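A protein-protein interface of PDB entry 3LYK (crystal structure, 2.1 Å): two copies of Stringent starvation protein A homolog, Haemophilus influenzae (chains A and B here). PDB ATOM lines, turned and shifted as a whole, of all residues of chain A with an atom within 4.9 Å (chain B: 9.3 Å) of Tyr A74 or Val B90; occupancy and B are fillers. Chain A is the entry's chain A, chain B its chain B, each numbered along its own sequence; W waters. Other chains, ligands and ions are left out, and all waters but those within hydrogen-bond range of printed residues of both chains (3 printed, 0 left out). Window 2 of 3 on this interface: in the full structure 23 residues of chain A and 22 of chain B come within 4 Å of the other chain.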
ATOM      1  N   LEU A  58     -10.306   4.842 -22.315  1.00  0.00           N
ATOM      2  CA  LEU A  58     -11.150   4.331 -21.267  1.00  0.00           C
ATOM      3  C   LEU A  58     -11.393   5.413 -20.260  1.00  0.00           C
ATOM      4  O   LEU A  58     -10.447   6.123 -19.896  1.00  0.00           O
ATOM      5  CB  LEU A  58     -10.487   3.117 -20.590  1.00  0.00           C
ATOM      6  CG  LEU A  58     -11.247   2.535 -19.396  1.00  0.00           C
ATOM      7  CD1 LEU A  58     -12.423   1.637 -19.897  1.00  0.00           C
ATOM      8  CD2 LEU A  58     -10.328   1.755 -18.445  1.00  0.00           C
ATOM      9  N   ASP A  60     -12.826   5.936 -16.408  1.00  0.00           N
ATOM     10  CA  ASP A  60     -13.209   5.243 -15.178  1.00  0.00           C
ATOM     11  C   ASP A  60     -13.418   6.283 -14.063  1.00  0.00           C
ATOM     12  O   ASP A  60     -12.434   6.886 -13.545  1.00  0.00           O
ATOM     13  CB  ASP A  60     -12.147   4.197 -14.784  1.00  0.00           C
ATOM     14  CG  ASP A  60     -12.517   3.421 -13.528  1.00  0.00           C
ATOM     15  OD1 ASP A  60     -13.592   3.679 -12.958  1.00  0.00           O
ATOM     16  OD2 ASP A  60     -11.747   2.531 -13.091  1.00  0.00           O
ATOM     17  N   LEU A  63     -10.952   9.175 -14.074  1.00  0.00           N
ATOM     18  CA  LEU A  63      -9.704   8.852 -14.757  1.00  0.00           C
ATOM     19  C   LEU A  63      -9.903   8.605 -16.253  1.00  0.00           C
ATOM     20  O   LEU A  63     -10.717   7.761 -16.643  1.00  0.00           O
ATOM     21  CB  LEU A  63      -9.107   7.605 -14.088  1.00  0.00           C
ATOM     22  CG  LEU A  63      -7.850   7.008 -14.735  1.00  0.00           C
ATOM     23  CD1 LEU A  63      -6.697   8.016 -14.585  1.00  0.00           C
ATOM     24  CD2 LEU A  63      -7.513   5.673 -14.097  1.00  0.00           C
ATOM     25  N   LEU A  65      -7.889   7.329 -19.664  1.00  0.00           N
ATOM     26  CA  LEU A  65      -6.692   6.628 -20.122  1.00  0.00           C
ATOM     27  C   LEU A  65      -6.714   6.320 -21.593  1.00  0.00           C
ATOM     28  O   LEU A  65      -7.770   6.026 -22.172  1.00  0.00           O
ATOM     29  CB  LEU A  65      -6.495   5.314 -19.363  1.00  0.00           C
ATOM     30  CG  LEU A  65      -6.258   5.305 -17.856  1.00  0.00           C
ATOM     31  CD1 LEU A  65      -6.039   3.875 -17.423  1.00  0.00           C
ATOM     32  CD2 LEU A  65      -5.002   6.193 -17.539  1.00  0.00           C
ATOM     33  N   ILE A  70      -1.287   0.790 -21.427  1.00  0.00           N
ATOM     34  CA  ILE A  70      -1.492   1.480 -20.151  1.00  0.00           C
ATOM     35  C   ILE A  70      -2.864   1.100 -19.545  1.00  0.00           C
ATOM     36  O   ILE A  70      -2.986   0.846 -18.339  1.00  0.00           O
ATOM     37  CB  ILE A  70      -1.350   3.003 -20.351  1.00  0.00           C
ATOM     38  CG1 ILE A  70       0.154   3.318 -20.570  1.00  0.00           C
ATOM     39  CG2 ILE A  70      -1.848   3.762 -19.157  1.00  0.00           C
ATOM     40  CD1 ILE A  70       0.456   4.764 -20.968  1.00  0.00           C
ATOM     41  N   ILE A  71      -3.877   1.019 -20.411  1.00  0.00           N
ATOM     42  CA  ILE A  71      -5.218   0.590 -19.993  1.00  0.00           C
ATOM     43  C   ILE A  71      -5.206  -0.818 -19.419  1.00  0.00           C
ATOM     44  O   ILE A  71      -5.733  -1.046 -18.354  1.00  0.00           O
ATOM     45  CB  ILE A  71      -6.192   0.669 -21.198  1.00  0.00           C
ATOM     46  CG1 ILE A  71      -6.407   2.151 -21.549  1.00  0.00           C
ATOM     47  CG2 ILE A  71      -7.544  -0.031 -20.865  1.00  0.00           C
ATOM     48  CD1 ILE A  71      -7.112   2.399 -22.883  1.00  0.00           C
ATOM     49  N   MET A  72      -4.598  -1.751 -20.136  1.00  0.00           N
ATOM     50  CA  MET A  72      -4.484  -3.121 -19.671  1.00  0.00           C
ATOM     51  C   MET A  72      -3.761  -3.280 -18.350  1.00  0.00           C
ATOM     52  O   MET A  72      -4.195  -4.045 -17.495  1.00  0.00           O
ATOM     53  CB  MET A  72      -3.834  -4.010 -20.757  1.00  0.00           C
ATOM     54  CG  MET A  72      -4.784  -4.190 -21.989  1.00  0.00           C
ATOM     55  SD  MET A  72      -4.042  -5.540 -23.196  1.00  0.00           S
ATOM     56  CE  MET A  72      -2.840  -4.419 -24.169  1.00  0.00           C
ATOM     57  N   GLU A  73      -2.673  -2.533 -18.166  1.00  0.00           N
ATOM     58  CA  GLU A  73      -1.933  -2.623 -16.923  1.00  0.00           C
ATOM     59  C   GLU A  73      -2.746  -2.015 -15.801  1.00  0.00           C
ATOM     60  O   GLU A  73      -2.822  -2.590 -14.728  1.00  0.00           O
ATOM     61  CB  GLU A  73      -0.518  -2.013 -17.088  1.00  0.00           C
ATOM     62  CG  GLU A  73       0.380  -2.961 -17.959  1.00  0.00           C
ATOM     63  CD  GLU A  73       1.793  -3.232 -17.379  1.00  0.00           C
ATOM     64  OE1 GLU A  73       1.926  -3.360 -16.134  1.00  0.00           O
ATOM     65  OE2 GLU A  73       2.764  -3.363 -18.176  1.00  0.00           O
ATOM     66  N   TYR A  74      -3.406  -0.885 -16.075  1.00  0.00           N
ATOM     67  CA  TYR A  74      -4.323  -0.309 -15.116  1.00  0.00           C
ATOM     68  C   TYR A  74      -5.435  -1.332 -14.692  1.00  0.00           C
ATOM     69  O   TYR A  74      -5.680  -1.561 -13.520  1.00  0.00           O
ATOM     70  CB  TYR A  74      -4.986   0.942 -15.719  1.00  0.00           C
ATOM     71  CG  TYR A  74      -6.115   1.408 -14.817  1.00  0.00           C
ATOM     72  CD1 TYR A  74      -5.841   1.907 -13.536  1.00  0.00           C
ATOM     73  CD2 TYR A  74      -7.457   1.286 -15.203  1.00  0.00           C
ATOM     74  CE1 TYR A  74      -6.866   2.311 -12.680  1.00  0.00           C
ATOM     75  CE2 TYR A  74      -8.530   1.687 -14.318  1.00  0.00           C
ATOM     76  CZ  TYR A  74      -8.217   2.176 -13.078  1.00  0.00           C
ATOM     77  OH  TYR A  74      -9.213   2.597 -12.209  1.00  0.00           O
ATOM     78  N   LEU A  75      -6.065  -1.969 -15.665  1.00  0.00           N
ATOM     79  CA  LEU A  75      -7.135  -2.951 -15.358  1.00  0.00           C
ATOM     80  C   LEU A  75      -6.579  -4.130 -14.540  1.00  0.00           C
ATOM     81  O   LEU A  75      -7.195  -4.574 -13.568  1.00  0.00           O
ATOM     82  CB  LEU A  75      -7.757  -3.474 -16.671  1.00  0.00           C
ATOM     83  CG  LEU A  75      -8.622  -2.396 -17.392  1.00  0.00           C
ATOM     84  CD1 LEU A  75      -9.113  -2.868 -18.774  1.00  0.00           C
ATOM     85  CD2 LEU A  75      -9.833  -1.853 -16.585  1.00  0.00           C
ATOM     86  N   ASP A  76      -5.399  -4.607 -14.910  1.00  0.00           N
ATOM     87  CA  ASP A  76      -4.821  -5.745 -14.184  1.00  0.00           C
ATOM     88  C   ASP A  76      -4.489  -5.365 -12.735  1.00  0.00           C
ATOM     89  O   ASP A  76      -4.582  -6.208 -11.827  1.00  0.00           O
ATOM     90  CB  ASP A  76      -3.563  -6.286 -14.877  1.00  0.00           C
ATOM     91  CG  ASP A  76      -3.210  -7.702 -14.393  1.00  0.00           C
ATOM     92  OD1 ASP A  76      -4.127  -8.573 -14.291  1.00  0.00           O
ATOM     93  OD2 ASP A  76      -2.022  -7.959 -14.095  1.00  0.00           O
ATOM     94  N   GLU A  77      -4.126  -4.102 -12.524  1.00  0.00           N
ATOM     95  CA  GLU A  77      -3.815  -3.628 -11.184  1.00  0.00           C
ATOM     96  C   GLU A  77      -5.034  -3.211 -10.408  1.00  0.00           C
ATOM     97  O   GLU A  77      -5.112  -3.475  -9.203  1.00  0.00           O
ATOM     98  CB  GLU A  77      -2.777  -2.472 -11.221  1.00  0.00           C
ATOM     99  CG  GLU A  77      -1.399  -2.966 -11.675  1.00  0.00           C
ATOM    100  CD  GLU A  77      -0.370  -1.805 -11.930  1.00  0.00           C
ATOM    101  OE1 GLU A  77      -0.703  -0.614 -11.822  1.00  0.00           O
ATOM    102  OE2 GLU A  77       0.766  -2.113 -12.274  1.00  0.00           O
ATOM    103  N   ARG A  78      -5.978  -2.537 -11.068  1.00  0.00           N
ATOM    104  CA  ARG A  78      -7.198  -2.117 -10.367  1.00  0.00           C
ATOM    105  C   ARG A  78      -8.086  -3.306  -9.993  1.00  0.00           C
ATOM    106  O   ARG A  78      -8.709  -3.309  -8.927  1.00  0.00           O
ATOM    107  CB  ARG A  78      -8.020  -1.142 -11.232  1.00  0.00           C
ATOM    108  CG  ARG A  78      -9.285  -0.587 -10.524  1.00  0.00           C
ATOM    109  CD  ARG A  78      -8.884   0.465  -9.492  1.00  0.00           C
ATOM    110  NE  ARG A  78      -9.734   0.589  -8.310  1.00  0.00           N
ATOM    111  CZ  ARG A  78     -10.914   1.203  -8.292  1.00  0.00           C
ATOM    112  NH1 ARG A  78     -11.392   1.702  -9.421  1.00  0.00           N
ATOM    113  NH2 ARG A  78     -11.631   1.319  -7.158  1.00  0.00           N
ATOM    114  N   PHE A  79      -8.168  -4.282 -10.896  1.00  0.00           N
ATOM    115  CA  PHE A  79      -9.058  -5.459 -10.712  1.00  0.00           C
ATOM    116  C   PHE A  79      -8.183  -6.695 -10.634  1.00  0.00           C
ATOM    117  O   PHE A  79      -7.887  -7.323 -11.640  1.00  0.00           O
ATOM    118  CB  PHE A  79     -10.106  -5.543 -11.853  1.00  0.00           C
ATOM    119  CG  PHE A  79     -10.895  -4.272 -12.004  1.00  0.00           C
ATOM    120  CD1 PHE A  79     -11.898  -3.944 -11.096  1.00  0.00           C
ATOM    121  CD2 PHE A  79     -10.631  -3.417 -13.036  1.00  0.00           C
ATOM    122  CE1 PHE A  79     -12.600  -2.750 -11.208  1.00  0.00           C
ATOM    123  CE2 PHE A  79     -11.303  -2.197 -13.151  1.00  0.00           C
ATOM    124  CZ  PHE A  79     -12.313  -1.873 -12.234  1.00  0.00           C
ATOM    125  N   GLU B  73      10.741  -0.402 -15.051  1.00  0.00           N
ATOM    126  CA  GLU B  73       9.725  -1.086 -14.256  1.00  0.00           C
ATOM    127  C   GLU B  73      10.250  -2.381 -13.689  1.00  0.00           C
ATOM    128  O   GLU B  73       9.964  -2.691 -12.560  1.00  0.00           O
ATOM    129  CB  GLU B  73       8.409  -1.275 -15.041  1.00  0.00           C
ATOM    130  CG  GLU B  73       7.633   0.089 -15.143  1.00  0.00           C
ATOM    131  CD  GLU B  73       6.079  -0.077 -15.202  1.00  0.00           C
ATOM    132  OE1 GLU B  73       5.515  -0.851 -14.357  1.00  0.00           O
ATOM    133  OE2 GLU B  73       5.452   0.589 -16.085  1.00  0.00           O
ATOM    134  N   GLN B  86       4.025   4.840  -7.215  1.00  0.00           N
ATOM    135  CA  GLN B  86       3.172   4.673  -6.046  1.00  0.00           C
ATOM    136  C   GLN B  86       2.621   3.296  -6.030  1.00  0.00           C
ATOM    137  O   GLN B  86       2.896   2.476  -6.895  1.00  0.00           O
ATOM    138  CB  GLN B  86       2.041   5.661  -6.083  1.00  0.00           C
ATOM    139  CG  GLN B  86       2.526   6.957  -6.600  1.00  0.00           C
ATOM    140  CD  GLN B  86       1.738   8.089  -6.065  1.00  0.00           C
ATOM    141  OE1 GLN B  86       1.067   7.973  -5.041  1.00  0.00           O
ATOM    142  NE2 GLN B  86       1.804   9.204  -6.749  1.00  0.00           N
ATOM    143  N   VAL B  87       1.825   3.068  -5.021  1.00  0.00           N
ATOM    144  CA  VAL B  87       1.339   1.756  -4.647  1.00  0.00           C
ATOM    145  C   VAL B  87      -0.011   1.490  -5.355  1.00  0.00           C
ATOM    146  O   VAL B  87      -0.305   0.367  -5.782  1.00  0.00           O
ATOM    147  CB  VAL B  87       1.194   1.779  -3.078  1.00  0.00           C
ATOM    148  CG1 VAL B  87       0.617   0.495  -2.518  1.00  0.00           C
ATOM    149  CG2 VAL B  87       2.615   2.060  -2.437  1.00  0.00           C
ATOM    150  N   TYR B  88      -0.802   2.541  -5.499  1.00  0.00           N
ATOM    151  CA  TYR B  88      -2.214   2.411  -5.844  1.00  0.00           C
ATOM    152  C   TYR B  88      -2.482   2.502  -7.356  1.00  0.00           C
ATOM    153  O   TYR B  88      -1.827   3.246  -8.057  1.00  0.00           O
ATOM    154  CB  TYR B  88      -3.037   3.426  -5.015  1.00  0.00           C
ATOM    155  CG  TYR B  88      -3.004   3.050  -3.555  1.00  0.00           C
ATOM    156  CD1 TYR B  88      -3.790   2.005  -3.076  1.00  0.00           C
ATOM    157  CD2 TYR B  88      -2.125   3.684  -2.657  1.00  0.00           C
ATOM    158  CE1 TYR B  88      -3.730   1.590  -1.740  1.00  0.00           C
ATOM    159  CE2 TYR B  88      -2.063   3.295  -1.289  1.00  0.00           C
ATOM    160  CZ  TYR B  88      -2.870   2.245  -0.841  1.00  0.00           C
ATOM    161  OH  TYR B  88      -2.839   1.860   0.488  1.00  0.00           O
ATOM    162  N   PRO B  89      -3.449   1.721  -7.865  1.00  0.00           N
ATOM    163  CA  PRO B  89      -3.503   1.623  -9.338  1.00  0.00           C
ATOM    164  C   PRO B  89      -3.836   2.901 -10.086  1.00  0.00           C
ATOM    165  O   PRO B  89      -3.353   3.046 -11.190  1.00  0.00           O
ATOM    166  CB  PRO B  89      -4.589   0.568  -9.614  1.00  0.00           C
ATOM    167  CG  PRO B  89      -5.230   0.274  -8.268  1.00  0.00           C
ATOM    168  CD  PRO B  89      -4.331   0.752  -7.182  1.00  0.00           C
ATOM    169  N   VAL B  90      -4.658   3.797  -9.533  1.00  0.00           N
ATOM    170  CA  VAL B  90      -4.985   5.034 -10.278  1.00  0.00           C
ATOM    171  C   VAL B  90      -3.724   5.955 -10.415  1.00  0.00           C
ATOM    172  O   VAL B  90      -3.447   6.489 -11.499  1.00  0.00           O
ATOM    173  CB  VAL B  90      -6.164   5.822  -9.635  1.00  0.00           C
ATOM    174  CG1 VAL B  90      -6.306   7.257 -10.289  1.00  0.00           C
ATOM    175  CG2 VAL B  90      -7.537   5.001  -9.750  1.00  0.00           C
ATOM    176  N   SER B  91      -2.980   6.147  -9.331  1.00  0.00           N
ATOM    177  CA  SER B  91      -1.722   6.941  -9.376  1.00  0.00           C
ATOM    178  C   SER B  91      -0.744   6.352 -10.344  1.00  0.00           C
ATOM    179  O   SER B  91      -0.055   7.096 -11.056  1.00  0.00           O
ATOM    180  CB  SER B  91      -1.001   6.899  -8.030  1.00  0.00           C
ATOM    181  OG  SER B  91      -1.812   7.509  -7.081  1.00  0.00           O
ATOM    182  N   ARG B  92      -0.627   5.016 -10.313  1.00  0.00           N
ATOM    183  CA  ARG B  92       0.299   4.334 -11.227  1.00  0.00           C
ATOM    184  C   ARG B  92      -0.077   4.578 -12.683  1.00  0.00           C
ATOM    185  O   ARG B  92       0.795   4.842 -13.531  1.00  0.00           O
ATOM    186  CB  ARG B  92       0.412   2.850 -10.891  1.00  0.00           C
ATOM    187  CG  ARG B  92       0.983   2.635  -9.464  1.00  0.00           C
ATOM    188  CD  ARG B  92       0.834   1.171  -9.019  1.00  0.00           C
ATOM    189  NE  ARG B  92       1.418   0.218  -9.959  1.00  0.00           N
ATOM    190  CZ  ARG B  92       2.688  -0.193  -9.931  1.00  0.00           C
ATOM    191  NH1 ARG B  92       3.544   0.322  -9.048  1.00  0.00           N
ATOM    192  NH2 ARG B  92       3.111  -1.102 -10.807  1.00  0.00           N
ATOM    193  N   ALA B  93      -1.394   4.548 -12.971  1.00  0.00           N
ATOM    194  CA  ALA B  93      -1.848   4.762 -14.351  1.00  0.00           C
ATOM    195  C   ALA B  93      -1.604   6.220 -14.766  1.00  0.00           C
ATOM    196  O   ALA B  93      -1.176   6.483 -15.869  1.00  0.00           O
ATOM    197  CB  ALA B  93      -3.362   4.424 -14.494  1.00  0.00           C
ATOM    198  N   LYS B  94      -1.907   7.164 -13.892  1.00  0.00           N
ATOM    199  CA  LYS B  94      -1.632   8.578 -14.240  1.00  0.00           C
ATOM    200  C   LYS B  94      -0.153   8.822 -14.505  1.00  0.00           C
ATOM    201  O   LYS B  94       0.181   9.490 -15.460  1.00  0.00           O
ATOM    202  CB  LYS B  94      -2.170   9.544 -13.194  1.00  0.00           C
ATOM    203  CG  LYS B  94      -3.660   9.334 -13.035  1.00  0.00           C
ATOM    204  CD  LYS B  94      -4.454  10.607 -13.059  1.00  0.00           C
ATOM    205  CE  LYS B  94      -5.069  10.795 -11.724  1.00  0.00           C
ATOM    206  NZ  LYS B  94      -4.045  10.229 -10.834  1.00  0.00           N
ATOM    207  N   ASP B  95       0.728   8.235 -13.695  1.00  0.00           N
ATOM    208  CA  ASP B  95       2.183   8.380 -13.938  1.00  0.00           C
ATOM    209  C   ASP B  95       2.622   7.765 -15.246  1.00  0.00           C
ATOM    210  O   ASP B  95       3.475   8.329 -15.960  1.00  0.00           O
ATOM    211  CB  ASP B  95       2.986   7.769 -12.792  1.00  0.00           C
ATOM    212  CG  ASP B  95       2.939   8.637 -11.553  1.00  0.00           C
ATOM    213  OD1 ASP B  95       2.408   9.774 -11.647  1.00  0.00           O
ATOM    214  OD2 ASP B  95       3.418   8.198 -10.496  1.00  0.00           O
ATOM    215  N   ARG B  96       2.073   6.592 -15.556  1.00  0.00           N
ATOM    216  CA  ARG B  96       2.370   5.947 -16.828  1.00  0.00           C
ATOM    217  C   ARG B  96       1.937   6.797 -18.012  1.00  0.00           C
ATOM    218  O   ARG B  96       2.636   6.871 -19.048  1.00  0.00           O
ATOM    219  CB  ARG B  96       1.723   4.548 -16.910  1.00  0.00           C
ATOM    220  CG  ARG B  96       2.480   3.460 -16.095  1.00  0.00           C
ATOM    221  CD  ARG B  96       2.031   2.081 -16.483  1.00  0.00           C
ATOM    222  NE  ARG B  96       2.704   1.078 -15.666  1.00  0.00           N
ATOM    223  CZ  ARG B  96       2.118   0.394 -14.681  1.00  0.00           C
ATOM    224  NH1 ARG B  96       0.822   0.598 -14.385  1.00  0.00           N
ATOM    225  NH2 ARG B  96       2.820  -0.520 -14.005  1.00  0.00           N
ATOM    226  N   LEU B  97       0.751   7.394 -17.891  1.00  0.00           N
ATOM    227  CA  LEU B  97       0.211   8.200 -18.995  1.00  0.00           C
ATOM    228  C   LEU B  97       1.050   9.482 -19.184  1.00  0.00           C
ATOM    229  O   LEU B  97       1.346   9.899 -20.311  1.00  0.00           O
ATOM    230  CB  LEU B  97      -1.248   8.559 -18.727  1.00  0.00           C
ATOM    231  CG  LEU B  97      -1.954   9.055 -19.998  1.00  0.00           C
ATOM    232  CD1 LEU B  97      -1.953   7.987 -21.058  1.00  0.00           C
ATOM    233  CD2 LEU B  97      -3.392   9.524 -19.724  1.00  0.00           C
ATOM    234  N   LEU B  98       1.441  10.075 -18.060  1.00  0.00           N
ATOM    235  CA  LEU B  98       2.339  11.239 -18.046  1.00  0.00           C
ATOM    236  C   LEU B  98       3.660  10.941 -18.745  1.00  0.00           C
ATOM    237  O   LEU B  98       4.123  11.714 -19.582  1.00  0.00           O
ATOM    238  CB  LEU B  98       2.581  11.628 -16.589  1.00  0.00           C
ATOM    239  CG  LEU B  98       2.880  13.038 -16.150  1.00  0.00           C
ATOM    240  CD1 LEU B  98       2.149  14.034 -17.050  1.00  0.00           C
ATOM    241  CD2 LEU B  98       2.365  13.142 -14.724  1.00  0.00           C
ATOM    242  N   ASN B 147       4.029  14.997  -8.559  1.00  0.00           N
ATOM    243  CA  ASN B 147       4.123  14.050  -7.461  1.00  0.00           C
ATOM    244  C   ASN B 147       4.774  14.692  -6.260  1.00  0.00           C
ATOM    245  O   ASN B 147       5.556  15.648  -6.400  1.00  0.00           O
ATOM    246  CB  ASN B 147       4.872  12.754  -7.865  1.00  0.00           C
ATOM    247  CG  ASN B 147       3.960  11.750  -8.618  1.00  0.00           C
ATOM    248  OD1 ASN B 147       3.017  11.221  -8.036  1.00  0.00           O
ATOM    249  ND2 ASN B 147       4.211  11.533  -9.911  1.00  0.00           N
HETATM  250  O   HOH W   1       4.427  -0.846 -18.471  1.00  0.00           O
HETATM  251  O   HOH W   2      -2.229   1.174 -12.825  1.00  0.00           O
HETATM  252  O   HOH W   3      -1.523   1.705 -15.879  1.00  0.00           O
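1 position is printed for both chains. Of the 12 pairs that touch across the chains among the printed residues, none has its exchanged pair printed and touching as well.
The guanidinium group (NE) of Arg B92 lies within salt-bridge range of the side-chain carboxylate (OE1) of Glu A77 (2.9 Å). NH2 of Arg B96 is in salt-bridge range of OE1 of Glu A73. The side-chain carboxylate (OE2) of Glu A77 is in salt-bridge range of the guanidinium group (NH2) of Arg B96 (3.1 Å).
The backbone NH of Leu A58 lies within hydrogen-bond range of the backbone carbonyl oxygen of Leu A65 (2.8 Å). OE1 of Glu B73 is in salt-bridge range of NH2 of Arg B96 (2.7 Å). NH1 of Arg A78 lies within salt-bridge range of OD2 of Asp A60 (3.8 Å). The side-chain carboxylate (OD2) of Asp A60 sits at hydrogen-bond distance from the side-chain hydroxyl (OH) of Tyr A74, at 2.7 Å. O of Gln B86 sits at hydrogen-bond distance from NH1 of Arg B92 (3.1 Å).
Tyr A74 touches just these residues of chain B: Pro B89, Val B90 and Ala B93. Val B90 touches just one residue of chain A: Tyr A74 (3.8 Å). Of the printed residues of chain B, Leu A65 touches Ala B93 (3.9 Å). Printed residues of chain B within 4 Å of Arg A78: Pro B89 (3.7 Å). Printed residues of chain B within 4 Å of Leu A63: Lys B94. Of the printed residues of chain A, Leu B97 touches Ile A70. Ser B91 touches none of the printed residues of chain A. The nearest residue of chain B that does not touch Tyr A74 is Arg B96 (4.8 Å). The nearest printed residue of chain A that does not touch Arg B92 is Glu A73 (5.9 Å).
Hydrophobic or aromatic side chains of chain A within 4 Å of the printed part of chain B: Leu A63, Leu A65, Ile A70 and Tyr A74. Along chain A the printed residues that touch a printed residue of chain B span positions 63 to 78. Among the printed residues, 12 pairs touch across the chains.
Among the printed residues, merely in contact across the chains: Ile A70 with Arg B96 (3.6 Å), Tyr A74 with Pro B89 (3.6 Å), Leu A63 with Lys B94 (3.7 Å), Tyr A74 with Ala B93 (3.7 Å), Arg A78 with Pro B89 (3.7 Å), Tyr A74 with Val B90 (3.8 Å), Glu A77 with Pro B89 (3.9 Å), Leu A65 with Ala B93 (3.9 Å) and Ile A70 with Leu B97 (3.97 Å).
Water W2 lies within hydrogen-bond range of the side-chain carboxylate of Glu A77 (2.6 Å), the backbone carbonyl oxygen of Pro B89 (2.7 Å), the guanidinium group of Arg B96 (3.5 Å) and the backbone NH of Ala B93 (3.5 Å). Water W1 bridges OE2 of Glu B73 and OE2 of Glu A73. Water W3 lies within hydrogen-bond range of the backbone carbonyl oxygen (O) of Ile A70, the guanidinium group (NH1) of Arg B96 and the backbone NH (N) of Tyr A74.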
